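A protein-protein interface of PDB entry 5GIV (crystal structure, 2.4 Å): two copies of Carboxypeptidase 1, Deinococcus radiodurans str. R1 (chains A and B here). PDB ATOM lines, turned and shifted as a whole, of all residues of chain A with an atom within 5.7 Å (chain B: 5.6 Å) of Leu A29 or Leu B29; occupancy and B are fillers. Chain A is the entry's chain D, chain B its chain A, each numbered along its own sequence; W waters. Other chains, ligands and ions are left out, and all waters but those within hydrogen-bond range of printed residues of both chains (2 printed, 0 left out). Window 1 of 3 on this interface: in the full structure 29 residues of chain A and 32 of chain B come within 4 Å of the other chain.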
ATOM      1  N   GLY A  24     -24.367 -25.667 -10.197  1.00  0.00           N
ATOM      2  CA  GLY A  24     -24.755 -24.578  -9.313  1.00  0.00           C
ATOM      3  C   GLY A  24     -23.942 -23.317  -9.536  1.00  0.00           C
ATOM      4  O   GLY A  24     -24.488 -22.212  -9.560  1.00  0.00           O
ATOM      5  N   GLY A  25     -22.623 -23.461  -9.696  1.00  0.00           N
ATOM      6  CA  GLY A  25     -21.787 -22.295  -9.947  1.00  0.00           C
ATOM      7  C   GLY A  25     -22.145 -21.598 -11.247  1.00  0.00           C
ATOM      8  O   GLY A  25     -22.123 -20.367 -11.338  1.00  0.00           O
ATOM      9  N   ILE A  26     -22.454 -22.377 -12.279  1.00  0.00           N
ATOM     10  CA  ILE A  26     -22.846 -21.793 -13.552  1.00  0.00           C
ATOM     11  C   ILE A  26     -24.191 -21.084 -13.413  1.00  0.00           C
ATOM     12  O   ILE A  26     -24.368 -19.962 -13.898  1.00  0.00           O
ATOM     13  CB  ILE A  26     -22.857 -22.889 -14.639  1.00  0.00           C
ATOM     14  CG1 ILE A  26     -21.452 -23.488 -14.771  1.00  0.00           C
ATOM     15  CG2 ILE A  26     -23.325 -22.337 -15.963  1.00  0.00           C
ATOM     16  CD1 ILE A  26     -21.344 -24.671 -15.687  1.00  0.00           C
ATOM     17  N   GLU A  27     -25.157 -21.721 -12.740  1.00  0.00           N
ATOM     18  CA  GLU A  27     -26.431 -21.060 -12.458  1.00  0.00           C
ATOM     19  C   GLU A  27     -26.228 -19.769 -11.681  1.00  0.00           C
ATOM     20  O   GLU A  27     -26.905 -18.767 -11.932  1.00  0.00           O
ATOM     21  CB  GLU A  27     -27.361 -21.995 -11.684  1.00  0.00           C
ATOM     22  CG  GLU A  27     -27.865 -23.173 -12.483  1.00  0.00           C
ATOM     23  CD  GLU A  27     -28.933 -23.956 -11.744  1.00  0.00           C
ATOM     24  OE1 GLU A  27     -28.591 -24.621 -10.738  1.00  0.00           O
ATOM     25  OE2 GLU A  27     -30.112 -23.892 -12.160  1.00  0.00           O
ATOM     26  N   ALA A  28     -25.315 -19.781 -10.711  1.00  0.00           N
ATOM     27  CA  ALA A  28     -25.059 -18.568  -9.948  1.00  0.00           C
ATOM     28  C   ALA A  28     -24.496 -17.473 -10.844  1.00  0.00           C
ATOM     29  O   ALA A  28     -24.792 -16.287 -10.650  1.00  0.00           O
ATOM     30  CB  ALA A  28     -24.110 -18.868  -8.785  1.00  0.00           C
ATOM     31  N   LEU A  29     -23.653 -17.851 -11.815  1.00  0.00           N
ATOM     32  CA  LEU A  29     -23.109 -16.866 -12.745  1.00  0.00           C
ATOM     33  C   LEU A  29     -24.216 -16.239 -13.593  1.00  0.00           C
ATOM     34  O   LEU A  29     -24.232 -15.019 -13.805  1.00  0.00           O
ATOM     35  CB  LEU A  29     -22.044 -17.512 -13.636  1.00  0.00           C
ATOM     36  CG  LEU A  29     -21.469 -16.638 -14.753  1.00  0.00           C
ATOM     37  CD1 LEU A  29     -20.815 -15.403 -14.183  1.00  0.00           C
ATOM     38  CD2 LEU A  29     -20.475 -17.421 -15.600  1.00  0.00           C
ATOM     39  N   LEU A  30     -25.161 -17.056 -14.069  1.00  0.00           N
ATOM     40  CA  LEU A  30     -26.271 -16.522 -14.853  1.00  0.00           C
ATOM     41  C   LEU A  30     -27.066 -15.503 -14.050  1.00  0.00           C
ATOM     42  O   LEU A  30     -27.467 -14.461 -14.581  1.00  0.00           O
ATOM     43  CB  LEU A  30     -27.170 -17.660 -15.331  1.00  0.00           C
ATOM     44  CG  LEU A  30     -26.626 -18.455 -16.517  1.00  0.00           C
ATOM     45  CD1 LEU A  30     -27.334 -19.791 -16.688  1.00  0.00           C
ATOM     46  CD2 LEU A  30     -26.763 -17.636 -17.787  1.00  0.00           C
ATOM     47  N   GLY A  31     -27.287 -15.776 -12.766  1.00  0.00           N
ATOM     48  CA  GLY A  31     -27.999 -14.852 -11.905  1.00  0.00           C
ATOM     49  C   GLY A  31     -27.175 -13.649 -11.500  1.00  0.00           C
ATOM     50  O   GLY A  31     -27.703 -12.536 -11.400  1.00  0.00           O
ATOM     51  N   TRP A  32     -25.887 -13.858 -11.229  1.00  0.00           N
ATOM     52  CA  TRP A  32     -25.020 -12.732 -10.891  1.00  0.00           C
ATOM     53  C   TRP A  32     -24.940 -11.749 -12.055  1.00  0.00           C
ATOM     54  O   TRP A  32     -25.093 -10.532 -11.877  1.00  0.00           O
ATOM     55  CB  TRP A  32     -23.625 -13.234 -10.513  1.00  0.00           C
ATOM     56  CG  TRP A  32     -22.615 -12.137 -10.328  1.00  0.00           C
ATOM     57  CD1 TRP A  32     -22.346 -11.461  -9.171  1.00  0.00           C
ATOM     58  CD2 TRP A  32     -21.736 -11.587 -11.322  1.00  0.00           C
ATOM     59  NE1 TRP A  32     -21.364 -10.529  -9.382  1.00  0.00           N
ATOM     60  CE2 TRP A  32     -20.964 -10.590 -10.691  1.00  0.00           C
ATOM     61  CE3 TRP A  32     -21.527 -11.841 -12.683  1.00  0.00           C
ATOM     62  CZ2 TRP A  32     -20.005  -9.836 -11.374  1.00  0.00           C
ATOM     63  CZ3 TRP A  32     -20.569 -11.094 -13.356  1.00  0.00           C
ATOM     64  CH2 TRP A  32     -19.818 -10.105 -12.698  1.00  0.00           C
ATOM     65  N   ASP A  33     -24.711 -12.266 -13.265  1.00  0.00           N
ATOM     66  CA  ASP A  33     -24.638 -11.389 -14.423  1.00  0.00           C
ATOM     67  C   ASP A  33     -25.980 -10.723 -14.686  1.00  0.00           C
ATOM     68  O   ASP A  33     -26.026  -9.551 -15.086  1.00  0.00           O
ATOM     69  CB  ASP A  33     -24.173 -12.184 -15.647  1.00  0.00           C
ATOM     70  CG  ASP A  33     -24.136 -11.347 -16.903  1.00  0.00           C
ATOM     71  OD1 ASP A  33     -23.181 -10.558 -17.062  1.00  0.00           O
ATOM     72  OD2 ASP A  33     -25.062 -11.486 -17.726  1.00  0.00           O
ATOM     73  N   GLN A  34     -27.078 -11.435 -14.426  1.00  0.00           N
ATOM     74  CA  GLN A  34     -28.396 -10.850 -14.625  1.00  0.00           C
ATOM     75  C   GLN A  34     -28.612  -9.624 -13.742  1.00  0.00           C
ATOM     76  O   GLN A  34     -29.238  -8.650 -14.174  1.00  0.00           O
ATOM     77  CB  GLN A  34     -29.486 -11.882 -14.356  1.00  0.00           C
ATOM     78  CG  GLN A  34     -30.860 -11.280 -14.497  1.00  0.00           C
ATOM     79  CD  GLN A  34     -31.908 -12.104 -13.840  1.00  0.00           C
ATOM     80  OE1 GLN A  34     -32.077 -12.033 -12.620  1.00  0.00           O
ATOM     81  NE2 GLN A  34     -32.624 -12.910 -14.626  1.00  0.00           N
ATOM     82  N   ARG A  46     -32.165 -14.613 -21.107  1.00  0.00           N
ATOM     83  CA  ARG A  46     -31.430 -15.047 -19.926  1.00  0.00           C
ATOM     84  C   ARG A  46     -32.284 -15.964 -19.059  1.00  0.00           C
ATOM     85  O   ARG A  46     -31.803 -16.999 -18.572  1.00  0.00           O
ATOM     86  CB  ARG A  46     -30.940 -13.835 -19.138  1.00  0.00           C
ATOM     87  CG  ARG A  46     -30.326 -14.188 -17.793  1.00  0.00           C
ATOM     88  CD  ARG A  46     -29.173 -15.185 -17.929  1.00  0.00           C
ATOM     89  NE  ARG A  46     -28.165 -14.754 -18.895  1.00  0.00           N
ATOM     90  CZ  ARG A  46     -27.168 -13.927 -18.607  1.00  0.00           C
ATOM     91  NH1 ARG A  46     -27.041 -13.445 -17.382  1.00  0.00           N
ATOM     92  NH2 ARG A  46     -26.297 -13.584 -19.542  1.00  0.00           N
ATOM     93  N   GLN A  49     -32.257 -19.297 -20.634  1.00  0.00           N
ATOM     94  CA  GLN A  49     -30.987 -19.942 -20.313  1.00  0.00           C
ATOM     95  C   GLN A  49     -31.003 -20.513 -18.902  1.00  0.00           C
ATOM     96  O   GLN A  49     -30.539 -21.638 -18.673  1.00  0.00           O
ATOM     97  CB  GLN A  49     -29.831 -18.956 -20.476  1.00  0.00           C
ATOM     98  CG  GLN A  49     -29.562 -18.551 -21.903  1.00  0.00           C
ATOM     99  CD  GLN A  49     -28.623 -17.377 -21.985  1.00  0.00           C
ATOM    100  OE1 GLN A  49     -28.302 -16.751 -20.971  1.00  0.00           O
ATOM    101  NE2 GLN A  49     -28.168 -17.069 -23.197  1.00  0.00           N
ATOM    102  N   THR A 239     -23.198 -14.135  -3.734  1.00  0.00           N
ATOM    103  CA  THR A 239     -23.477 -15.354  -4.483  1.00  0.00           C
ATOM    104  C   THR A 239     -22.173 -16.091  -4.766  1.00  0.00           C
ATOM    105  O   THR A 239     -21.133 -15.463  -4.987  1.00  0.00           O
ATOM    106  CB  THR A 239     -24.257 -15.048  -5.773  1.00  0.00           C
ATOM    107  OG1 THR A 239     -24.563 -16.272  -6.466  1.00  0.00           O
ATOM    108  CG2 THR A 239     -23.480 -14.128  -6.664  1.00  0.00           C
ATOM    109  N   LEU A 241     -20.065 -18.456  -7.121  1.00  0.00           N
ATOM    110  CA  LEU A 241     -19.922 -18.944  -8.485  1.00  0.00           C
ATOM    111  C   LEU A 241     -18.953 -20.117  -8.600  1.00  0.00           C
ATOM    112  O   LEU A 241     -18.781 -20.665  -9.699  1.00  0.00           O
ATOM    113  CB  LEU A 241     -19.463 -17.798  -9.395  1.00  0.00           C
ATOM    114  CG  LEU A 241     -20.522 -16.733  -9.721  1.00  0.00           C
ATOM    115  CD1 LEU A 241     -21.043 -16.049  -8.459  1.00  0.00           C
ATOM    116  CD2 LEU A 241     -20.000 -15.699 -10.710  1.00  0.00           C
ATOM    117  N   ARG A 247     -18.780 -13.803  -4.704  1.00  0.00           N
ATOM    118  CA  ARG A 247     -18.895 -12.400  -5.081  1.00  0.00           C
ATOM    119  C   ARG A 247     -19.986 -11.692  -4.284  1.00  0.00           C
ATOM    120  O   ARG A 247     -21.015 -12.281  -3.942  1.00  0.00           O
ATOM    121  CB  ARG A 247     -19.201 -12.264  -6.575  1.00  0.00           C
ATOM    122  CG  ARG A 247     -18.276 -13.075  -7.435  1.00  0.00           C
ATOM    123  CD  ARG A 247     -18.319 -12.665  -8.879  1.00  0.00           C
ATOM    124  NE  ARG A 247     -17.488 -13.553  -9.682  1.00  0.00           N
ATOM    125  CZ  ARG A 247     -17.425 -13.522 -11.005  1.00  0.00           C
ATOM    126  NH1 ARG A 247     -18.144 -12.625 -11.676  1.00  0.00           N
ATOM    127  NH2 ARG A 247     -16.647 -14.384 -11.652  1.00  0.00           N
ATOM    128  N   GLY B  24     -24.841 -22.064 -26.385  1.00  0.00           N
ATOM    129  CA  GLY B  24     -23.833 -21.163 -26.916  1.00  0.00           C
ATOM    130  C   GLY B  24     -23.744 -19.858 -26.152  1.00  0.00           C
ATOM    131  O   GLY B  24     -22.650 -19.355 -25.894  1.00  0.00           O
ATOM    132  N   GLY B  25     -24.893 -19.275 -25.805  1.00  0.00           N
ATOM    133  CA  GLY B  25     -24.871 -18.058 -25.011  1.00  0.00           C
ATOM    134  C   GLY B  25     -24.257 -18.277 -23.640  1.00  0.00           C
ATOM    135  O   GLY B  25     -23.480 -17.450 -23.159  1.00  0.00           O
ATOM    136  N   ILE B  26     -24.587 -19.405 -22.999  1.00  0.00           N
ATOM    137  CA  ILE B  26     -24.051 -19.690 -21.670  1.00  0.00           C
ATOM    138  C   ILE B  26     -22.554 -19.952 -21.734  1.00  0.00           C
ATOM    139  O   ILE B  26     -21.787 -19.437 -20.908  1.00  0.00           O
ATOM    140  CB  ILE B  26     -24.802 -20.865 -21.022  1.00  0.00           C
ATOM    141  CG1 ILE B  26     -26.282 -20.524 -20.849  1.00  0.00           C
ATOM    142  CG2 ILE B  26     -24.170 -21.213 -19.691  1.00  0.00           C
ATOM    143  CD1 ILE B  26     -27.100 -21.671 -20.326  1.00  0.00           C
ATOM    144  N   GLU B  27     -22.107 -20.748 -22.708  1.00  0.00           N
ATOM    145  CA  GLU B  27     -20.671 -20.933 -22.887  1.00  0.00           C
ATOM    146  C   GLU B  27     -19.981 -19.591 -23.084  1.00  0.00           C
ATOM    147  O   GLU B  27     -18.891 -19.355 -22.550  1.00  0.00           O
ATOM    148  CB  GLU B  27     -20.399 -21.864 -24.070  1.00  0.00           C
ATOM    149  CG  GLU B  27     -20.825 -23.304 -23.846  1.00  0.00           C
ATOM    150  CD  GLU B  27     -20.383 -24.234 -24.969  1.00  0.00           C
ATOM    151  OE1 GLU B  27     -19.206 -24.664 -24.970  1.00  0.00           O
ATOM    152  OE2 GLU B  27     -21.216 -24.528 -25.857  1.00  0.00           O
ATOM    153  N   ALA B  28     -20.613 -18.695 -23.842  1.00  0.00           N
ATOM    154  CA  ALA B  28     -20.039 -17.374 -24.076  1.00  0.00           C
ATOM    155  C   ALA B  28     -19.980 -16.565 -22.790  1.00  0.00           C
ATOM    156  O   ALA B  28     -19.010 -15.835 -22.551  1.00  0.00           O
ATOM    157  CB  ALA B  28     -20.851 -16.642 -25.151  1.00  0.00           C
ATOM    158  N   LEU B  29     -21.008 -16.682 -21.948  1.00  0.00           N
ATOM    159  CA  LEU B  29     -20.998 -15.978 -20.670  1.00  0.00           C
ATOM    160  C   LEU B  29     -19.855 -16.461 -19.792  1.00  0.00           C
ATOM    161  O   LEU B  29     -19.195 -15.662 -19.128  1.00  0.00           O
ATOM    162  CB  LEU B  29     -22.334 -16.161 -19.947  1.00  0.00           C
ATOM    163  CG  LEU B  29     -22.389 -15.593 -18.525  1.00  0.00           C
ATOM    164  CD1 LEU B  29     -22.091 -14.101 -18.532  1.00  0.00           C
ATOM    165  CD2 LEU B  29     -23.745 -15.879 -17.888  1.00  0.00           C
ATOM    166  N   LEU B  30     -19.623 -17.768 -19.761  1.00  0.00           N
ATOM    167  CA  LEU B  30     -18.516 -18.294 -18.971  1.00  0.00           C
ATOM    168  C   LEU B  30     -17.189 -17.742 -19.464  1.00  0.00           C
ATOM    169  O   LEU B  30     -16.304 -17.429 -18.663  1.00  0.00           O
ATOM    170  CB  LEU B  30     -18.517 -19.817 -19.025  1.00  0.00           C
ATOM    171  CG  LEU B  30     -19.576 -20.514 -18.184  1.00  0.00           C
ATOM    172  CD1 LEU B  30     -19.714 -21.964 -18.660  1.00  0.00           C
ATOM    173  CD2 LEU B  30     -19.219 -20.444 -16.698  1.00  0.00           C
ATOM    174  N   GLY B  31     -17.028 -17.628 -20.785  1.00  0.00           N
ATOM    175  CA  GLY B  31     -15.798 -17.073 -21.327  1.00  0.00           C
ATOM    176  C   GLY B  31     -15.707 -15.566 -21.173  1.00  0.00           C
ATOM    177  O   GLY B  31     -14.635 -15.025 -20.872  1.00  0.00           O
ATOM    178  N   TRP B  32     -16.824 -14.864 -21.378  1.00  0.00           N
ATOM    179  CA  TRP B  32     -16.805 -13.414 -21.206  1.00  0.00           C
ATOM    180  C   TRP B  32     -16.439 -13.044 -19.776  1.00  0.00           C
ATOM    181  O   TRP B  32     -15.594 -12.171 -19.547  1.00  0.00           O
ATOM    182  CB  TRP B  32     -18.158 -12.816 -21.589  1.00  0.00           C
ATOM    183  CG  TRP B  32     -18.291 -11.360 -21.219  1.00  0.00           C
ATOM    184  CD1 TRP B  32     -17.953 -10.279 -21.982  1.00  0.00           C
ATOM    185  CD2 TRP B  32     -18.810 -10.838 -19.991  1.00  0.00           C
ATOM    186  NE1 TRP B  32     -18.238  -9.112 -21.307  1.00  0.00           N
ATOM    187  CE2 TRP B  32     -18.764  -9.431 -20.082  1.00  0.00           C
ATOM    188  CE3 TRP B  32     -19.314 -11.427 -18.823  1.00  0.00           C
ATOM    189  CZ2 TRP B  32     -19.189  -8.603 -19.045  1.00  0.00           C
ATOM    190  CZ3 TRP B  32     -19.741 -10.603 -17.795  1.00  0.00           C
ATOM    191  CH2 TRP B  32     -19.677  -9.205 -17.913  1.00  0.00           C
ATOM    192  N   ASP B  33     -17.065 -13.705 -18.799  1.00  0.00           N
ATOM    193  CA  ASP B  33     -16.749 -13.428 -17.404  1.00  0.00           C
ATOM    194  C   ASP B  33     -15.316 -13.824 -17.072  1.00  0.00           C
ATOM    195  O   ASP B  33     -14.644 -13.142 -16.286  1.00  0.00           O
ATOM    196  CB  ASP B  33     -17.749 -14.159 -16.498  1.00  0.00           C
ATOM    197  CG  ASP B  33     -17.427 -14.006 -15.015  1.00  0.00           C
ATOM    198  OD1 ASP B  33     -17.728 -12.932 -14.435  1.00  0.00           O
ATOM    199  OD2 ASP B  33     -16.866 -14.968 -14.442  1.00  0.00           O
ATOM    200  N   GLN B  34     -14.821 -14.903 -17.685  1.00  0.00           N
ATOM    201  CA  GLN B  34     -13.444 -15.323 -17.455  1.00  0.00           C
ATOM    202  C   GLN B  34     -12.456 -14.233 -17.844  1.00  0.00           C
ATOM    203  O   GLN B  34     -11.421 -14.060 -17.193  1.00  0.00           O
ATOM    204  CB  GLN B  34     -13.166 -16.606 -18.231  1.00  0.00           C
ATOM    205  CG  GLN B  34     -11.739 -17.090 -18.162  1.00  0.00           C
ATOM    206  CD  GLN B  34     -11.439 -18.140 -19.212  1.00  0.00           C
ATOM    207  OE1 GLN B  34     -11.792 -17.993 -20.392  1.00  0.00           O
ATOM    208  NE2 GLN B  34     -10.808 -19.226 -18.786  1.00  0.00           N
ATOM    209  N   ARG B  46     -13.368 -22.530 -13.107  1.00  0.00           N
ATOM    210  CA  ARG B  46     -14.053 -22.030 -14.285  1.00  0.00           C
ATOM    211  C   ARG B  46     -13.763 -22.914 -15.492  1.00  0.00           C
ATOM    212  O   ARG B  46     -14.656 -23.172 -16.306  1.00  0.00           O
ATOM    213  CB  ARG B  46     -13.652 -20.578 -14.552  1.00  0.00           C
ATOM    214  CG  ARG B  46     -14.225 -20.015 -15.837  1.00  0.00           C
ATOM    215  CD  ARG B  46     -15.762 -20.061 -15.874  1.00  0.00           C
ATOM    216  NE  ARG B  46     -16.385 -19.441 -14.710  1.00  0.00           N
ATOM    217  CZ  ARG B  46     -16.616 -18.134 -14.582  1.00  0.00           C
ATOM    218  NH1 ARG B  46     -16.279 -17.294 -15.556  1.00  0.00           N
ATOM    219  NH2 ARG B  46     -17.187 -17.663 -13.477  1.00  0.00           N
ATOM    220  N   LEU B 241     -23.591 -13.234 -26.003  1.00  0.00           N
ATOM    221  CA  LEU B 241     -24.096 -14.010 -24.874  1.00  0.00           C
ATOM    222  C   LEU B 241     -25.565 -14.375 -25.028  1.00  0.00           C
ATOM    223  O   LEU B 241     -26.108 -15.071 -24.161  1.00  0.00           O
ATOM    224  CB  LEU B 241     -23.883 -13.256 -23.554  1.00  0.00           C
ATOM    225  CG  LEU B 241     -22.452 -13.242 -23.005  1.00  0.00           C
ATOM    226  CD1 LEU B 241     -21.457 -12.639 -23.995  1.00  0.00           C
ATOM    227  CD2 LEU B 241     -22.369 -12.503 -21.668  1.00  0.00           C
ATOM    228  N   ARG B 247     -21.766  -8.310 -26.624  1.00  0.00           N
ATOM    229  CA  ARG B 247     -20.878  -7.518 -25.786  1.00  0.00           C
ATOM    230  C   ARG B 247     -19.516  -7.321 -26.440  1.00  0.00           C
ATOM    231  O   ARG B 247     -19.021  -8.181 -27.174  1.00  0.00           O
ATOM    232  CB  ARG B 247     -20.720  -8.176 -24.418  1.00  0.00           C
ATOM    233  CG  ARG B 247     -22.064  -8.504 -23.787  1.00  0.00           C
ATOM    234  CD  ARG B 247     -21.953  -8.766 -22.293  1.00  0.00           C
ATOM    235  NE  ARG B 247     -23.249  -9.132 -21.730  1.00  0.00           N
ATOM    236  CZ  ARG B 247     -23.446  -9.541 -20.479  1.00  0.00           C
ATOM    237  NH1 ARG B 247     -22.430  -9.640 -19.628  1.00  0.00           N
ATOM    238  NH2 ARG B 247     -24.666  -9.849 -20.078  1.00  0.00           N
HETATM  239  O   HOH W   1     -27.127 -13.254 -22.299  1.00  0.00           O
HETATM  240  O   HOH W   2     -16.608 -18.830 -11.031  1.00  0.00           O
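The side-chain carboxylate (OD1) of Asp B33 is in salt-bridge range of the guanidinium group (NH1) of Arg A247 (2.8 Å).
The side-chain amide nitrogen (NE2) of Gln A49 sits at hydrogen-bond distance from the backbone carbonyl oxygen (O) of Leu B241 (3.0 Å).
The guanidinium group of Arg B247 is in salt-bridge range of the side-chain carboxylate of Asp A33 (2.8 Å).
The guanidinium group (NH1) of Arg B46 is in hydrogen-bond range of the backbone carbonyl oxygen (O) of Leu B30 (3.1 Å).
The guanidinium group (NH1) of Arg B46 is in salt-bridge range of the side-chain carboxylate (OD2) of Asp B33, 2.6 Å away.
O of Leu A30 lies within hydrogen-bond range of NH1 of Arg A46 (3.0 Å).
OD2 of Asp A33 is in salt-bridge range of NH1 of Arg A46, 2.8 Å away.
The guanidinium group (NE) of Arg A46 is in hydrogen-bond range of the side-chain amide oxygen (OE1) of Gln A49.
N of Thr A239 is in hydrogen-bond range of O of Arg A247 (2.9 Å).
Among the printed residues, merely in contact across the chains: Leu A29 with Leu B30, Leu A30 with Leu B29, Asp A33 with Trp B32, Trp A32 with Asp B33, Leu A29 with Asp B33, Arg A247 with Arg B46, Asp A33 with Leu B29, Arg A46 with Leu B29, Gln A49 with Ile B26, Gln A49 with Gly B25, Leu A29 with Arg B46, Leu A29 with Leu B29 and Ile A26 with Ile B26.
Gly A24 touches none of the printed residues of chain B.
Printed residues of chain B within 4 Å of Leu A29: Leu B29, Leu B30, Asp B33 and Arg B46.
Of the printed residues of chain B, Trp A32 touches Asp B33.
Of the printed residues of chain B, Gln A49 touches Gly B25, Ile B26 and Leu B241.
Leu B29 touches just these residues of chain A: Leu A29, Leu A30, Asp A33 and Arg A46.
Of the printed residues of chain A, Asp B33 touches Leu A29 (3.8 Å), Trp A32 (3.6 Å) and Arg A247 (2.8 Å).
Of the printed residues of chain A, Leu B241 touches Gln A49 (3.0 Å).
The nearest residue of chain A that does not touch Leu B29 is Gln A49 (5.6 Å).
The nearest printed residue of chain B that does not touch Ile A26 is Leu B30 (4.2 Å).
Of the 14 printed residues of chain B, 9 touch a printed residue of chain A.
Hydrophobic or aromatic side chains of chain B within 4 Å of the printed part of chain A: Ile B26, Leu B29, Leu B30 and Trp B32.
Among the printed residues, 16 pairs touch across the chains.
Among the printed residues, Asp or Glu carboxylates within 4 Å of a Lys or Arg side-chain nitrogen of the other chain: Asp A33 with Arg B247 (2.8 Å) and Arg A247 with Asp B33 (2.8 Å).
Leu A29 touches Leu B30, and with the chains exchanged Leu A30 touches Leu B29.
Leu A29 touches Asp B33, and with the chains exchanged Asp A33 touches Leu B29.
Asp A33 touches Arg B247, and with the chains exchanged Arg A247 touches Asp B33.
Arg A247 touches Arg B46, but with the chains exchanged Arg A46 does not touch Arg B247 (4.1 Å).
Of the 16 pairs that touch across the chains among the printed residues, 12 have their exchanged pair printed and touching as well.
Water W2 lies within hydrogen-bond range of the guanidinium group (NH2) of Arg B46 (2.8 Å) and the backbone carbonyl oxygen (O) of Leu A241 (3.1 Å).
Water W1 bridges the backbone carbonyl oxygen (O) of Leu B241 (2.8 Å) and the guanidinium group (NH2) of Arg A46 (2.9 Å).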
